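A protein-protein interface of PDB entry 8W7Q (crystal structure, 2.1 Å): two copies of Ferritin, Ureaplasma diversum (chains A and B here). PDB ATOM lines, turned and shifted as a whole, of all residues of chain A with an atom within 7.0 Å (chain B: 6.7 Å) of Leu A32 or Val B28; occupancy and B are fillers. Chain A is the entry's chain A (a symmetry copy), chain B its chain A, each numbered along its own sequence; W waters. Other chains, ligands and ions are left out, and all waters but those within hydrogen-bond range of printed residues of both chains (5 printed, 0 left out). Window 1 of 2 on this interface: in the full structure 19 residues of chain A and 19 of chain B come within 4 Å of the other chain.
Water W4 lies within hydrogen-bond range of the backbone carbonyl oxygen (O) of Val A88 (2.7 Å) and the backbone NH (N) of Thr B82 (2.9 Å).
Water W1 lies within hydrogen-bond range of OH of Tyr B24 (2.7 Å), OG1 of Thr B82 (2.8 Å) and O of Leu A32 (2.9 Å).
Water W3 bridges OG of Ser A58 (2.8 Å) and NZ of Lys B66 (2.9 Å).
Water W5 lies within hydrogen-bond range of O of Val A84 (2.8 Å) and O of Val B86 (3.3 Å).
Water W2 bridges the backbone carbonyl oxygen (O) of Val B84 (2.8 Å) and the backbone carbonyl oxygen (O) of Val A86 (3.3 Å).
Among the printed residues, pairs that only touch across the chains: Ser A85 with Val B84, Leu A32 with Val B28, Val A28 with Leu B32 and Val A84 with Val B84.
OE1 of Glu A29 is in hydrogen-bond range of N of Ser A85 (2.8 Å).
The side-chain hydroxyl of Thr B82 lies within hydrogen-bond range of a ring nitrogen (ND1) of His A36 (2.6 Å).
The backbone carbonyl oxygen (O) of Thr B82 is in hydrogen-bond range of the backbone NH (N) of Val A88, 2.9 Å away.
The backbone NH (N) of Val B84 sits at hydrogen-bond distance from the backbone carbonyl oxygen (O) of Val A86, at 2.8 Å.
The backbone carbonyl oxygen of Val B86 is in hydrogen-bond range of the backbone NH of Val A84 (2.8 Å).
Val A28 touches Leu B32, and with the chains exchanged Leu A32 touches Val B28.
Val B84 touches its own counterpart, Val A84.
Val A84 touches Val B86, and with the chains exchanged Val A86 touches Val B84.
Positions printed for both chains: 26, 27, 28, 29, 30, 31, 32, 33, 58, 61, 62, 84 and 86.
Leu A32 touches just one residue of chain B: Val B28.
Of the printed residues of chain B, Ser A85 touches Val B84 (3.3 Å).
Val B28 touches just one residue of chain A: Leu A32 (3.7 Å).
Printed residues of chain A within 4 Å of Val B84: Val A84 (3.9 Å), Ser A85 (3.3 Å) and Val A86 (2.8 Å).
Printed residues of chain A within 4 Å of Val B86: Val A84.
The nearest residue of chain A that does not touch Val B28 is Val A84 (6.4 Å).
Hydrophobic or aromatic side chains of chain B that line the printed part of chain A: Val B28, Leu B32 and Val B84.
Printed residues of chain A that touch a printed residue of chain B: Val A28, Leu A32, His A36, Val A84, Ser A85, Val A86 and Val A88.
Hydrophobic or aromatic side chains of chain A within 4 Å of the printed part of chain B: Val A28, Leu A32, His A36, Val A84 and Val A88.
Among the printed residues, 8 pairs touch across the chains.
Among the printed residues, no Asp or Glu carboxylate lies within 4 Å of a Lys or Arg side-chain nitrogen of the other chain.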
ATOM      1  N   LEU A  26     -12.876  -6.009 -15.546  1.00  0.00           N
ATOM      2  CA  LEU A  26     -11.775  -5.173 -16.017  1.00  0.00           C
ATOM      3  C   LEU A  26     -12.019  -3.708 -15.675  1.00  0.00           C
ATOM      4  O   LEU A  26     -11.101  -3.001 -15.244  1.00  0.00           O
ATOM      5  CB  LEU A  26     -11.595  -5.354 -17.531  1.00  0.00           C
ATOM      6  CG  LEU A  26     -10.572  -4.436 -18.228  1.00  0.00           C
ATOM      7  CD1 LEU A  26      -9.148  -4.877 -17.917  1.00  0.00           C
ATOM      8  CD2 LEU A  26     -10.778  -4.414 -19.730  1.00  0.00           C
ATOM      9  N   ASN A  27     -13.258  -3.233 -15.849  1.00  0.00           N
ATOM     10  CA  ASN A  27     -13.537  -1.825 -15.577  1.00  0.00           C
ATOM     11  C   ASN A  27     -13.478  -1.519 -14.090  1.00  0.00           C
ATOM     12  O   ASN A  27     -13.047  -0.431 -13.688  1.00  0.00           O
ATOM     13  CB  ASN A  27     -14.891  -1.445 -16.151  1.00  0.00           C
ATOM     14  CG  ASN A  27     -14.803  -1.082 -17.608  1.00  0.00           C
ATOM     15  OD1 ASN A  27     -14.250  -0.046 -17.958  1.00  0.00           O
ATOM     16  ND2 ASN A  27     -15.322  -1.948 -18.472  1.00  0.00           N
ATOM     17  N   VAL A  28     -13.912  -2.456 -13.251  1.00  0.00           N
ATOM     18  CA  VAL A  28     -13.775  -2.250 -11.815  1.00  0.00           C
ATOM     19  C   VAL A  28     -12.304  -2.157 -11.441  1.00  0.00           C
ATOM     20  O   VAL A  28     -11.866  -1.202 -10.786  1.00  0.00           O
ATOM     21  CB  VAL A  28     -14.482  -3.373 -11.040  1.00  0.00           C
ATOM     22  CG1 VAL A  28     -13.986  -3.382  -9.598  1.00  0.00           C
ATOM     23  CG2 VAL A  28     -15.989  -3.173 -11.109  1.00  0.00           C
ATOM     24  N   GLU A  29     -11.513  -3.146 -11.862  1.00  0.00           N
ATOM     25  CA  GLU A  29     -10.117  -3.199 -11.436  1.00  0.00           C
ATOM     26  C   GLU A  29      -9.315  -2.047 -12.023  1.00  0.00           C
ATOM     27  O   GLU A  29      -8.480  -1.449 -11.331  1.00  0.00           O
ATOM     28  CB  GLU A  29      -9.528  -4.563 -11.808  1.00  0.00           C
ATOM     29  CG  GLU A  29     -10.264  -5.654 -11.039  1.00  0.00           C
ATOM     30  CD  GLU A  29      -9.833  -7.069 -11.369  1.00  0.00           C
ATOM     31  OE1 GLU A  29     -10.233  -7.972 -10.601  1.00  0.00           O
ATOM     32  OE2 GLU A  29      -9.136  -7.291 -12.387  1.00  0.00           O
ATOM     33  N   LEU A  30      -9.572  -1.702 -13.286  1.00  0.00           N
ATOM     34  CA  LEU A  30      -8.942  -0.523 -13.872  1.00  0.00           C
ATOM     35  C   LEU A  30      -9.284   0.723 -13.074  1.00  0.00           C
ATOM     36  O   LEU A  30      -8.419   1.570 -12.812  1.00  0.00           O
ATOM     37  CB  LEU A  30      -9.407  -0.345 -15.313  1.00  0.00           C
ATOM     38  CG  LEU A  30      -8.530  -0.747 -16.481  1.00  0.00           C
ATOM     39  CD1 LEU A  30      -9.194  -0.199 -17.738  1.00  0.00           C
ATOM     40  CD2 LEU A  30      -7.140  -0.188 -16.301  1.00  0.00           C
ATOM     41  N   GLY A  31     -10.555   0.872 -12.710  1.00  0.00           N
ATOM     42  CA  GLY A  31     -10.956   2.060 -11.975  1.00  0.00           C
ATOM     43  C   GLY A  31     -10.228   2.167 -10.655  1.00  0.00           C
ATOM     44  O   GLY A  31      -9.828   3.257 -10.236  1.00  0.00           O
ATOM     45  N   LEU A  32     -10.014   1.029  -9.999  1.00  0.00           N
ATOM     46  CA  LEU A  32      -9.327   1.043  -8.714  1.00  0.00           C
ATOM     47  C   LEU A  32      -7.852   1.387  -8.880  1.00  0.00           C
ATOM     48  O   LEU A  32      -7.274   2.095  -8.042  1.00  0.00           O
ATOM     49  CB  LEU A  32      -9.505  -0.305  -8.024  1.00  0.00           C
ATOM     50  CG  LEU A  32     -10.959  -0.494  -7.580  1.00  0.00           C
ATOM     51  CD1 LEU A  32     -11.232  -1.923  -7.100  1.00  0.00           C
ATOM     52  CD2 LEU A  32     -11.263   0.497  -6.492  1.00  0.00           C
ATOM     53  N   VAL A  33      -7.229   0.893  -9.959  1.00  0.00           N
ATOM     54  CA  VAL A  33      -5.833   1.217 -10.228  1.00  0.00           C
ATOM     55  C   VAL A  33      -5.697   2.690 -10.574  1.00  0.00           C
ATOM     56  O   VAL A  33      -4.789   3.378 -10.090  1.00  0.00           O
ATOM     57  CB  VAL A  33      -5.287   0.324 -11.355  1.00  0.00           C
ATOM     58  CG1 VAL A  33      -3.949   0.853 -11.861  1.00  0.00           C
ATOM     59  CG2 VAL A  33      -5.157  -1.118 -10.868  1.00  0.00           C
ATOM     60  N   TYR A  34      -6.593   3.196 -11.418  1.00  0.00           N
ATOM     61  CA  TYR A  34      -6.540   4.606 -11.776  1.00  0.00           C
ATOM     62  C   TYR A  34      -6.697   5.488 -10.542  1.00  0.00           C
ATOM     63  O   TYR A  34      -6.016   6.513 -10.421  1.00  0.00           O
ATOM     64  CB  TYR A  34      -7.606   4.924 -12.824  1.00  0.00           C
ATOM     65  CG  TYR A  34      -7.312   4.377 -14.210  1.00  0.00           C
ATOM     66  CD1 TYR A  34      -6.076   3.831 -14.530  1.00  0.00           C
ATOM     67  CD2 TYR A  34      -8.279   4.410 -15.201  1.00  0.00           C
ATOM     68  CE1 TYR A  34      -5.820   3.332 -15.801  1.00  0.00           C
ATOM     69  CE2 TYR A  34      -8.034   3.913 -16.464  1.00  0.00           C
ATOM     70  CZ  TYR A  34      -6.808   3.383 -16.764  1.00  0.00           C
ATOM     71  OH  TYR A  34      -6.589   2.899 -18.038  1.00  0.00           O
ATOM     72  N   ALA A  35      -7.562   5.092  -9.595  1.00  0.00           N
ATOM     73  CA  ALA A  35      -7.702   5.891  -8.376  1.00  0.00           C
ATOM     74  C   ALA A  35      -6.383   5.950  -7.622  1.00  0.00           C
ATOM     75  O   ALA A  35      -6.031   6.985  -7.052  1.00  0.00           O
ATOM     76  CB  ALA A  35      -8.795   5.336  -7.463  1.00  0.00           C
ATOM     77  N   HIS A  36      -5.635   4.847  -7.617  1.00  0.00           N
ATOM     78  CA  HIS A  36      -4.322   4.865  -6.986  1.00  0.00           C
ATOM     79  C   HIS A  36      -3.368   5.752  -7.771  1.00  0.00           C
ATOM     80  O   HIS A  36      -2.679   6.601  -7.194  1.00  0.00           O
ATOM     81  CB  HIS A  36      -3.764   3.445  -6.880  1.00  0.00           C
ATOM     82  CG  HIS A  36      -2.655   3.316  -5.895  1.00  0.00           C
ATOM     83  ND1 HIS A  36      -2.815   2.697  -4.674  1.00  0.00           N
ATOM     84  CD2 HIS A  36      -1.372   3.750  -5.937  1.00  0.00           C
ATOM     85  CE1 HIS A  36      -1.676   2.754  -4.004  1.00  0.00           C
ATOM     86  NE2 HIS A  36      -0.784   3.387  -4.749  1.00  0.00           N
ATOM     87  N   TYR A  37      -3.333   5.576  -9.093  1.00  0.00           N
ATOM     88  CA  TYR A  37      -2.477   6.400  -9.939  1.00  0.00           C
ATOM     89  C   TYR A  37      -2.787   7.884  -9.778  1.00  0.00           C
ATOM     90  O   TYR A  37      -1.877   8.714  -9.842  1.00  0.00           O
ATOM     91  CB  TYR A  37      -2.624   5.988 -11.401  1.00  0.00           C
ATOM     92  CG  TYR A  37      -1.946   4.687 -11.776  1.00  0.00           C
ATOM     93  CD1 TYR A  37      -1.300   3.902 -10.819  1.00  0.00           C
ATOM     94  CD2 TYR A  37      -1.947   4.241 -13.096  1.00  0.00           C
ATOM     95  CE1 TYR A  37      -0.678   2.709 -11.170  1.00  0.00           C
ATOM     96  CE2 TYR A  37      -1.329   3.062 -13.453  1.00  0.00           C
ATOM     97  CZ  TYR A  37      -0.697   2.299 -12.487  1.00  0.00           C
ATOM     98  OH  TYR A  37      -0.089   1.121 -12.850  1.00  0.00           O
ATOM     99  N   SER A  58     -10.793   7.226 -13.654  1.00  0.00           N
ATOM    100  CA  SER A  58     -11.150   6.219 -12.655  1.00  0.00           C
ATOM    101  C   SER A  58     -12.658   6.170 -12.432  1.00  0.00           C
ATOM    102  O   SER A  58     -13.271   5.094 -12.464  1.00  0.00           O
ATOM    103  CB  SER A  58     -10.422   6.535 -11.347  1.00  0.00           C
ATOM    104  OG  SER A  58     -10.899   5.721 -10.301  1.00  0.00           O
ATOM    105  N   LYS A  61     -14.579   4.606 -15.345  1.00  0.00           N
ATOM    106  CA  LYS A  61     -14.560   3.141 -15.402  1.00  0.00           C
ATOM    107  C   LYS A  61     -15.436   2.537 -14.311  1.00  0.00           C
ATOM    108  O   LYS A  61     -16.194   1.589 -14.560  1.00  0.00           O
ATOM    109  CB  LYS A  61     -13.135   2.603 -15.258  1.00  0.00           C
ATOM    110  CG  LYS A  61     -12.107   3.152 -16.248  1.00  0.00           C
ATOM    111  CD  LYS A  61     -12.530   2.924 -17.690  1.00  0.00           C
ATOM    112  CE  LYS A  61     -11.452   3.409 -18.649  1.00  0.00           C
ATOM    113  NZ  LYS A  61     -11.781   3.101 -20.068  1.00  0.00           N
ATOM    114  N   LEU A  62     -15.329   3.053 -13.093  1.00  0.00           N
ATOM    115  CA  LEU A  62     -16.147   2.556 -11.999  1.00  0.00           C
ATOM    116  C   LEU A  62     -17.588   3.016 -12.082  1.00  0.00           C
ATOM    117  O   LEU A  62     -18.395   2.584 -11.257  1.00  0.00           O
ATOM    118  CB  LEU A  62     -15.559   2.988 -10.663  1.00  0.00           C
ATOM    119  CG  LEU A  62     -14.354   2.165 -10.234  1.00  0.00           C
ATOM    120  CD1 LEU A  62     -13.577   2.915  -9.190  1.00  0.00           C
ATOM    121  CD2 LEU A  62     -14.834   0.825  -9.704  1.00  0.00           C
ATOM    122  N   VAL A  84     -13.485  -9.716  -7.889  1.00  0.00           N
ATOM    123  CA  VAL A  84     -12.571  -8.597  -8.045  1.00  0.00           C
ATOM    124  C   VAL A  84     -11.319  -8.878  -7.240  1.00  0.00           C
ATOM    125  O   VAL A  84     -11.397  -9.185  -6.046  1.00  0.00           O
ATOM    126  CB  VAL A  84     -13.221  -7.280  -7.586  1.00  0.00           C
ATOM    127  CG1 VAL A  84     -12.179  -6.155  -7.542  1.00  0.00           C
ATOM    128  CG2 VAL A  84     -14.382  -6.936  -8.515  1.00  0.00           C
ATOM    129  N   SER A  85     -10.170  -8.769  -7.896  1.00  0.00           N
ATOM    130  CA  SER A  85      -8.880  -9.000  -7.258  1.00  0.00           C
ATOM    131  C   SER A  85      -7.878  -8.066  -7.916  1.00  0.00           C
ATOM    132  O   SER A  85      -7.547  -8.252  -9.087  1.00  0.00           O
ATOM    133  CB  SER A  85      -8.443 -10.452  -7.420  1.00  0.00           C
ATOM    134  OG  SER A  85      -7.083 -10.600  -7.064  1.00  0.00           O
ATOM    135  N   VAL A  86      -7.378  -7.083  -7.177  1.00  0.00           N
ATOM    136  CA  VAL A  86      -6.398  -6.176  -7.754  1.00  0.00           C
ATOM    137  C   VAL A  86      -5.550  -5.581  -6.639  1.00  0.00           C
ATOM    138  O   VAL A  86      -6.051  -5.225  -5.568  1.00  0.00           O
ATOM    139  CB  VAL A  86      -7.089  -5.099  -8.627  1.00  0.00           C
ATOM    140  CG1 VAL A  86      -7.893  -4.112  -7.779  1.00  0.00           C
ATOM    141  CG2 VAL A  86      -6.060  -4.384  -9.498  1.00  0.00           C
ATOM    142  N   VAL A  88      -2.046  -2.914  -6.212  1.00  0.00           N
ATOM    143  CA  VAL A  88      -1.084  -2.019  -6.846  1.00  0.00           C
ATOM    144  C   VAL A  88       0.248  -2.234  -6.132  1.00  0.00           C
ATOM    145  O   VAL A  88       0.491  -1.697  -5.051  1.00  0.00           O
ATOM    146  CB  VAL A  88      -1.538  -0.561  -6.792  1.00  0.00           C
ATOM    147  CG1 VAL A  88      -0.447   0.351  -7.351  1.00  0.00           C
ATOM    148  CG2 VAL A  88      -2.853  -0.391  -7.576  1.00  0.00           C
ATOM    149  N   HIS B  23      -9.367   0.685   6.322  1.00  0.00           N
ATOM    150  CA  HIS B  23     -10.693   1.254   6.154  1.00  0.00           C
ATOM    151  C   HIS B  23     -10.945   1.674   4.705  1.00  0.00           C
ATOM    152  O   HIS B  23     -12.073   1.564   4.216  1.00  0.00           O
ATOM    153  CB  HIS B  23     -10.886   2.427   7.112  1.00  0.00           C
ATOM    154  CG  HIS B  23     -12.320   2.706   7.399  1.00  0.00           C
ATOM    155  ND1 HIS B  23     -13.130   1.809   8.057  1.00  0.00           N
ATOM    156  CD2 HIS B  23     -13.110   3.753   7.056  1.00  0.00           C
ATOM    157  CE1 HIS B  23     -14.353   2.303   8.135  1.00  0.00           C
ATOM    158  NE2 HIS B  23     -14.367   3.483   7.538  1.00  0.00           N
ATOM    159  N   TYR B  24      -9.907   2.135   4.003  1.00  0.00           N
ATOM    160  CA  TYR B  24     -10.021   2.360   2.565  1.00  0.00           C
ATOM    161  C   TYR B  24     -10.463   1.088   1.861  1.00  0.00           C
ATOM    162  O   TYR B  24     -11.406   1.091   1.059  1.00  0.00           O
ATOM    163  CB  TYR B  24      -8.670   2.841   2.032  1.00  0.00           C
ATOM    164  CG  TYR B  24      -8.618   3.223   0.569  1.00  0.00           C
ATOM    165  CD1 TYR B  24      -8.860   4.529   0.171  1.00  0.00           C
ATOM    166  CD2 TYR B  24      -8.274   2.291  -0.403  1.00  0.00           C
ATOM    167  CE1 TYR B  24      -8.797   4.895  -1.156  1.00  0.00           C
ATOM    168  CE2 TYR B  24      -8.204   2.648  -1.738  1.00  0.00           C
ATOM    169  CZ  TYR B  24      -8.472   3.953  -2.105  1.00  0.00           C
ATOM    170  OH  TYR B  24      -8.402   4.320  -3.424  1.00  0.00           O
ATOM    171  N   LYS B  25      -9.768  -0.012   2.149  1.00  0.00           N
ATOM    172  CA  LYS B  25     -10.085  -1.309   1.570  1.00  0.00           C
ATOM    173  C   LYS B  25     -11.527  -1.709   1.866  1.00  0.00           C
ATOM    174  O   LYS B  25     -12.253  -2.168   0.979  1.00  0.00           O
ATOM    175  CB  LYS B  25      -9.091  -2.337   2.129  1.00  0.00           C
ATOM    176  CG  LYS B  25      -9.281  -3.782   1.721  1.00  0.00           C
ATOM    177  CD  LYS B  25      -8.192  -4.639   2.390  1.00  0.00           C
ATOM    178  CE  LYS B  25      -8.548  -6.114   2.383  1.00  0.00           C
ATOM    179  NZ  LYS B  25      -8.511  -6.657   0.988  1.00  0.00           N
ATOM    180  N   LEU B  26     -11.946  -1.563   3.121  1.00  0.00           N
ATOM    181  CA  LEU B  26     -13.308  -1.937   3.495  1.00  0.00           C
ATOM    182  C   LEU B  26     -14.330  -1.153   2.681  1.00  0.00           C
ATOM    183  O   LEU B  26     -15.330  -1.715   2.219  1.00  0.00           O
ATOM    184  CB  LEU B  26     -13.517  -1.703   4.998  1.00  0.00           C
ATOM    185  CG  LEU B  26     -14.944  -1.905   5.544  1.00  0.00           C
ATOM    186  CD1 LEU B  26     -15.285  -3.386   5.638  1.00  0.00           C
ATOM    187  CD2 LEU B  26     -15.113  -1.260   6.906  1.00  0.00           C
ATOM    188  N   ASN B  27     -14.092   0.148   2.482  1.00  0.00           N
ATOM    189  CA  ASN B  27     -15.061   0.955   1.745  1.00  0.00           C
ATOM    190  C   ASN B  27     -15.087   0.591   0.270  1.00  0.00           C
ATOM    191  O   ASN B  27     -16.148   0.620  -0.367  1.00  0.00           O
ATOM    192  CB  ASN B  27     -14.753   2.432   1.928  1.00  0.00           C
ATOM    193  CG  ASN B  27     -15.354   2.978   3.194  1.00  0.00           C
ATOM    194  OD1 ASN B  27     -16.567   3.115   3.297  1.00  0.00           O
ATOM    195  ND2 ASN B  27     -14.510   3.269   4.179  1.00  0.00           N
ATOM    196  N   VAL B  28     -13.934   0.252  -0.301  1.00  0.00           N
ATOM    197  CA  VAL B  28     -13.928  -0.208  -1.684  1.00  0.00           C
ATOM    198  C   VAL B  28     -14.725  -1.498  -1.807  1.00  0.00           C
ATOM    199  O   VAL B  28     -15.635  -1.614  -2.638  1.00  0.00           O
ATOM    200  CB  VAL B  28     -12.487  -0.389  -2.185  1.00  0.00           C
ATOM    201  CG1 VAL B  28     -12.493  -1.248  -3.445  1.00  0.00           C
ATOM    202  CG2 VAL B  28     -11.860   0.974  -2.444  1.00  0.00           C
ATOM    203  N   GLU B  29     -14.402  -2.485  -0.971  1.00  0.00           N
ATOM    204  CA  GLU B  29     -15.029  -3.797  -1.110  1.00  0.00           C
ATOM    205  C   GLU B  29     -16.513  -3.739  -0.777  1.00  0.00           C
ATOM    206  O   GLU B  29     -17.334  -4.364  -1.463  1.00  0.00           O
ATOM    207  CB  GLU B  29     -14.280  -4.810  -0.239  1.00  0.00           C
ATOM    208  CG  GLU B  29     -12.850  -4.949  -0.749  1.00  0.00           C
ATOM    209  CD  GLU B  29     -11.967  -5.867   0.072  1.00  0.00           C
ATOM    210  OE1 GLU B  29     -10.872  -6.197  -0.438  1.00  0.00           O
ATOM    211  OE2 GLU B  29     -12.331  -6.234   1.213  1.00  0.00           O
ATOM    212  N   LEU B  30     -16.881  -2.976   0.254  1.00  0.00           N
ATOM    213  CA  LEU B  30     -18.294  -2.763   0.546  1.00  0.00           C
ATOM    214  C   LEU B  30     -19.005  -2.142  -0.644  1.00  0.00           C
ATOM    215  O   LEU B  30     -20.122  -2.542  -1.000  1.00  0.00           O
ATOM    216  CB  LEU B  30     -18.445  -1.850   1.758  1.00  0.00           C
ATOM    217  CG  LEU B  30     -18.782  -2.404   3.128  1.00  0.00           C
ATOM    218  CD1 LEU B  30     -19.100  -1.210   4.018  1.00  0.00           C
ATOM    219  CD2 LEU B  30     -19.955  -3.348   3.028  1.00  0.00           C
ATOM    220  N   GLY B  31     -18.386  -1.133  -1.251  1.00  0.00           N
ATOM    221  CA  GLY B  31     -19.027  -0.471  -2.374  1.00  0.00           C
ATOM    222  C   GLY B  31     -19.275  -1.430  -3.515  1.00  0.00           C
ATOM    223  O   GLY B  31     -20.318  -1.379  -4.174  1.00  0.00           O
ATOM    224  N   LEU B  32     -18.334  -2.343  -3.741  1.00  0.00           N
ATOM    225  CA  LEU B  32     -18.488  -3.302  -4.827  1.00  0.00           C
ATOM    226  C   LEU B  32     -19.589  -4.310  -4.521  1.00  0.00           C
ATOM    227  O   LEU B  32     -20.338  -4.715  -5.423  1.00  0.00           O
ATOM    228  CB  LEU B  32     -17.157  -4.000  -5.088  1.00  0.00           C
ATOM    229  CG  LEU B  32     -16.149  -3.022  -5.697  1.00  0.00           C
ATOM    230  CD1 LEU B  32     -14.736  -3.614  -5.753  1.00  0.00           C
ATOM    231  CD2 LEU B  32     -16.617  -2.641  -7.073  1.00  0.00           C
ATOM    232  N   VAL B  33     -19.700  -4.725  -3.252  1.00  0.00           N
ATOM    233  CA  VAL B  33     -20.760  -5.644  -2.857  1.00  0.00           C
ATOM    234  C   VAL B  33     -22.112  -4.960  -2.965  1.00  0.00           C
ATOM    235  O   VAL B  33     -23.082  -5.538  -3.472  1.00  0.00           O
ATOM    236  CB  VAL B  33     -20.508  -6.168  -1.433  1.00  0.00           C
ATOM    237  CG1 VAL B  33     -21.749  -6.871  -0.890  1.00  0.00           C
ATOM    238  CG2 VAL B  33     -19.300  -7.101  -1.420  1.00  0.00           C
ATOM    239  N   SER B  58     -23.682   2.335  -2.370  1.00  0.00           N
ATOM    240  CA  SER B  58     -22.485   1.850  -3.056  1.00  0.00           C
ATOM    241  C   SER B  58     -21.599   3.006  -3.511  1.00  0.00           C
ATOM    242  O   SER B  58     -20.388   3.018  -3.256  1.00  0.00           O
ATOM    243  CB  SER B  58     -22.907   0.992  -4.250  1.00  0.00           C
ATOM    244  OG  SER B  58     -21.797   0.682  -5.060  1.00  0.00           O
ATOM    245  N   LYS B  61     -19.787   4.762  -0.638  1.00  0.00           N
ATOM    246  CA  LYS B  61     -18.595   4.076  -0.130  1.00  0.00           C
ATOM    247  C   LYS B  61     -17.437   4.181  -1.116  1.00  0.00           C
ATOM    248  O   LYS B  61     -16.292   4.442  -0.723  1.00  0.00           O
ATOM    249  CB  LYS B  61     -18.885   2.600   0.149  1.00  0.00           C
ATOM    250  CG  LYS B  61     -20.060   2.313   1.084  1.00  0.00           C
ATOM    251  CD  LYS B  61     -19.896   3.001   2.429  1.00  0.00           C
ATOM    252  CE  LYS B  61     -21.040   2.632   3.364  1.00  0.00           C
ATOM    253  NZ  LYS B  61     -20.856   3.198   4.729  1.00  0.00           N
ATOM    254  N   LEU B  62     -17.710   3.959  -2.396  1.00  0.00           N
ATOM    255  CA  LEU B  62     -16.672   4.065  -3.407  1.00  0.00           C
ATOM    256  C   LEU B  62     -16.298   5.500  -3.722  1.00  0.00           C
ATOM    257  O   LEU B  62     -15.365   5.710  -4.501  1.00  0.00           O
ATOM    258  CB  LEU B  62     -17.111   3.369  -4.689  1.00  0.00           C
ATOM    259  CG  LEU B  62     -16.998   1.854  -4.626  1.00  0.00           C
ATOM    260  CD1 LEU B  62     -17.852   1.240  -5.698  1.00  0.00           C
ATOM    261  CD2 LEU B  62     -15.540   1.459  -4.792  1.00  0.00           C
ATOM    262  N   LYS B  66     -13.876   6.655   0.487  1.00  0.00           N
ATOM    263  CA  LYS B  66     -12.499   6.300   0.167  1.00  0.00           C
ATOM    264  C   LYS B  66     -11.673   7.518  -0.219  1.00  0.00           C
ATOM    265  O   LYS B  66     -10.495   7.595   0.143  1.00  0.00           O
ATOM    266  CB  LYS B  66     -12.468   5.214  -0.928  1.00  0.00           C
ATOM    267  CG  LYS B  66     -12.420   5.671  -2.405  1.00  0.00           C
ATOM    268  CD  LYS B  66     -12.279   4.451  -3.329  1.00  0.00           C
ATOM    269  CE  LYS B  66     -11.838   4.786  -4.747  1.00  0.00           C
ATOM    270  NZ  LYS B  66     -12.574   5.961  -5.314  1.00  0.00           N
ATOM    271  N   THR B  82      -3.411   0.045  -2.253  1.00  0.00           N
ATOM    272  CA  THR B  82      -4.565  -0.516  -2.951  1.00  0.00           C
ATOM    273  C   THR B  82      -4.387  -2.025  -3.011  1.00  0.00           C
ATOM    274  O   THR B  82      -3.527  -2.528  -3.743  1.00  0.00           O
ATOM    275  CB  THR B  82      -4.709   0.072  -4.356  1.00  0.00           C
ATOM    276  OG1 THR B  82      -5.019   1.464  -4.256  1.00  0.00           O
ATOM    277  CG2 THR B  82      -5.814  -0.634  -5.135  1.00  0.00           C
ATOM    278  N   VAL B  84      -7.221  -5.160  -3.001  1.00  0.00           N
ATOM    279  CA  VAL B  84      -8.663  -5.343  -3.042  1.00  0.00           C
ATOM    280  C   VAL B  84      -8.959  -6.760  -3.490  1.00  0.00           C
ATOM    281  O   VAL B  84      -8.455  -7.208  -4.526  1.00  0.00           O
ATOM    282  CB  VAL B  84      -9.326  -4.330  -3.991  1.00  0.00           C
ATOM    283  CG1 VAL B  84     -10.806  -4.679  -4.197  1.00  0.00           C
ATOM    284  CG2 VAL B  84      -9.152  -2.921  -3.430  1.00  0.00           C
ATOM    285  N   VAL B  86     -12.536  -9.200  -3.418  1.00  0.00           N
ATOM    286  CA  VAL B  86     -13.910  -9.407  -2.987  1.00  0.00           C
ATOM    287  C   VAL B  86     -14.661 -10.174  -4.067  1.00  0.00           C
ATOM    288  O   VAL B  86     -14.502  -9.923  -5.265  1.00  0.00           O
ATOM    289  CB  VAL B  86     -14.584  -8.061  -2.624  1.00  0.00           C
ATOM    290  CG1 VAL B  86     -14.825  -7.194  -3.861  1.00  0.00           C
ATOM    291  CG2 VAL B  86     -15.877  -8.309  -1.851  1.00  0.00           C
HETATM  292  O   HOH W   1      -7.384   2.552  -5.198  1.00  0.00           O
HETATM  293  O   HOH W   2      -5.837  -8.200  -4.104  1.00  0.00           O
HETATM  294  O   HOH W   3     -12.564   6.328  -8.168  1.00  0.00           O
HETATM  295  O   HOH W   4      -0.679  -0.587  -2.929  1.00  0.00           O
HETATM  296  O   HOH W   5     -11.900 -11.947  -5.679  1.00  0.00           O
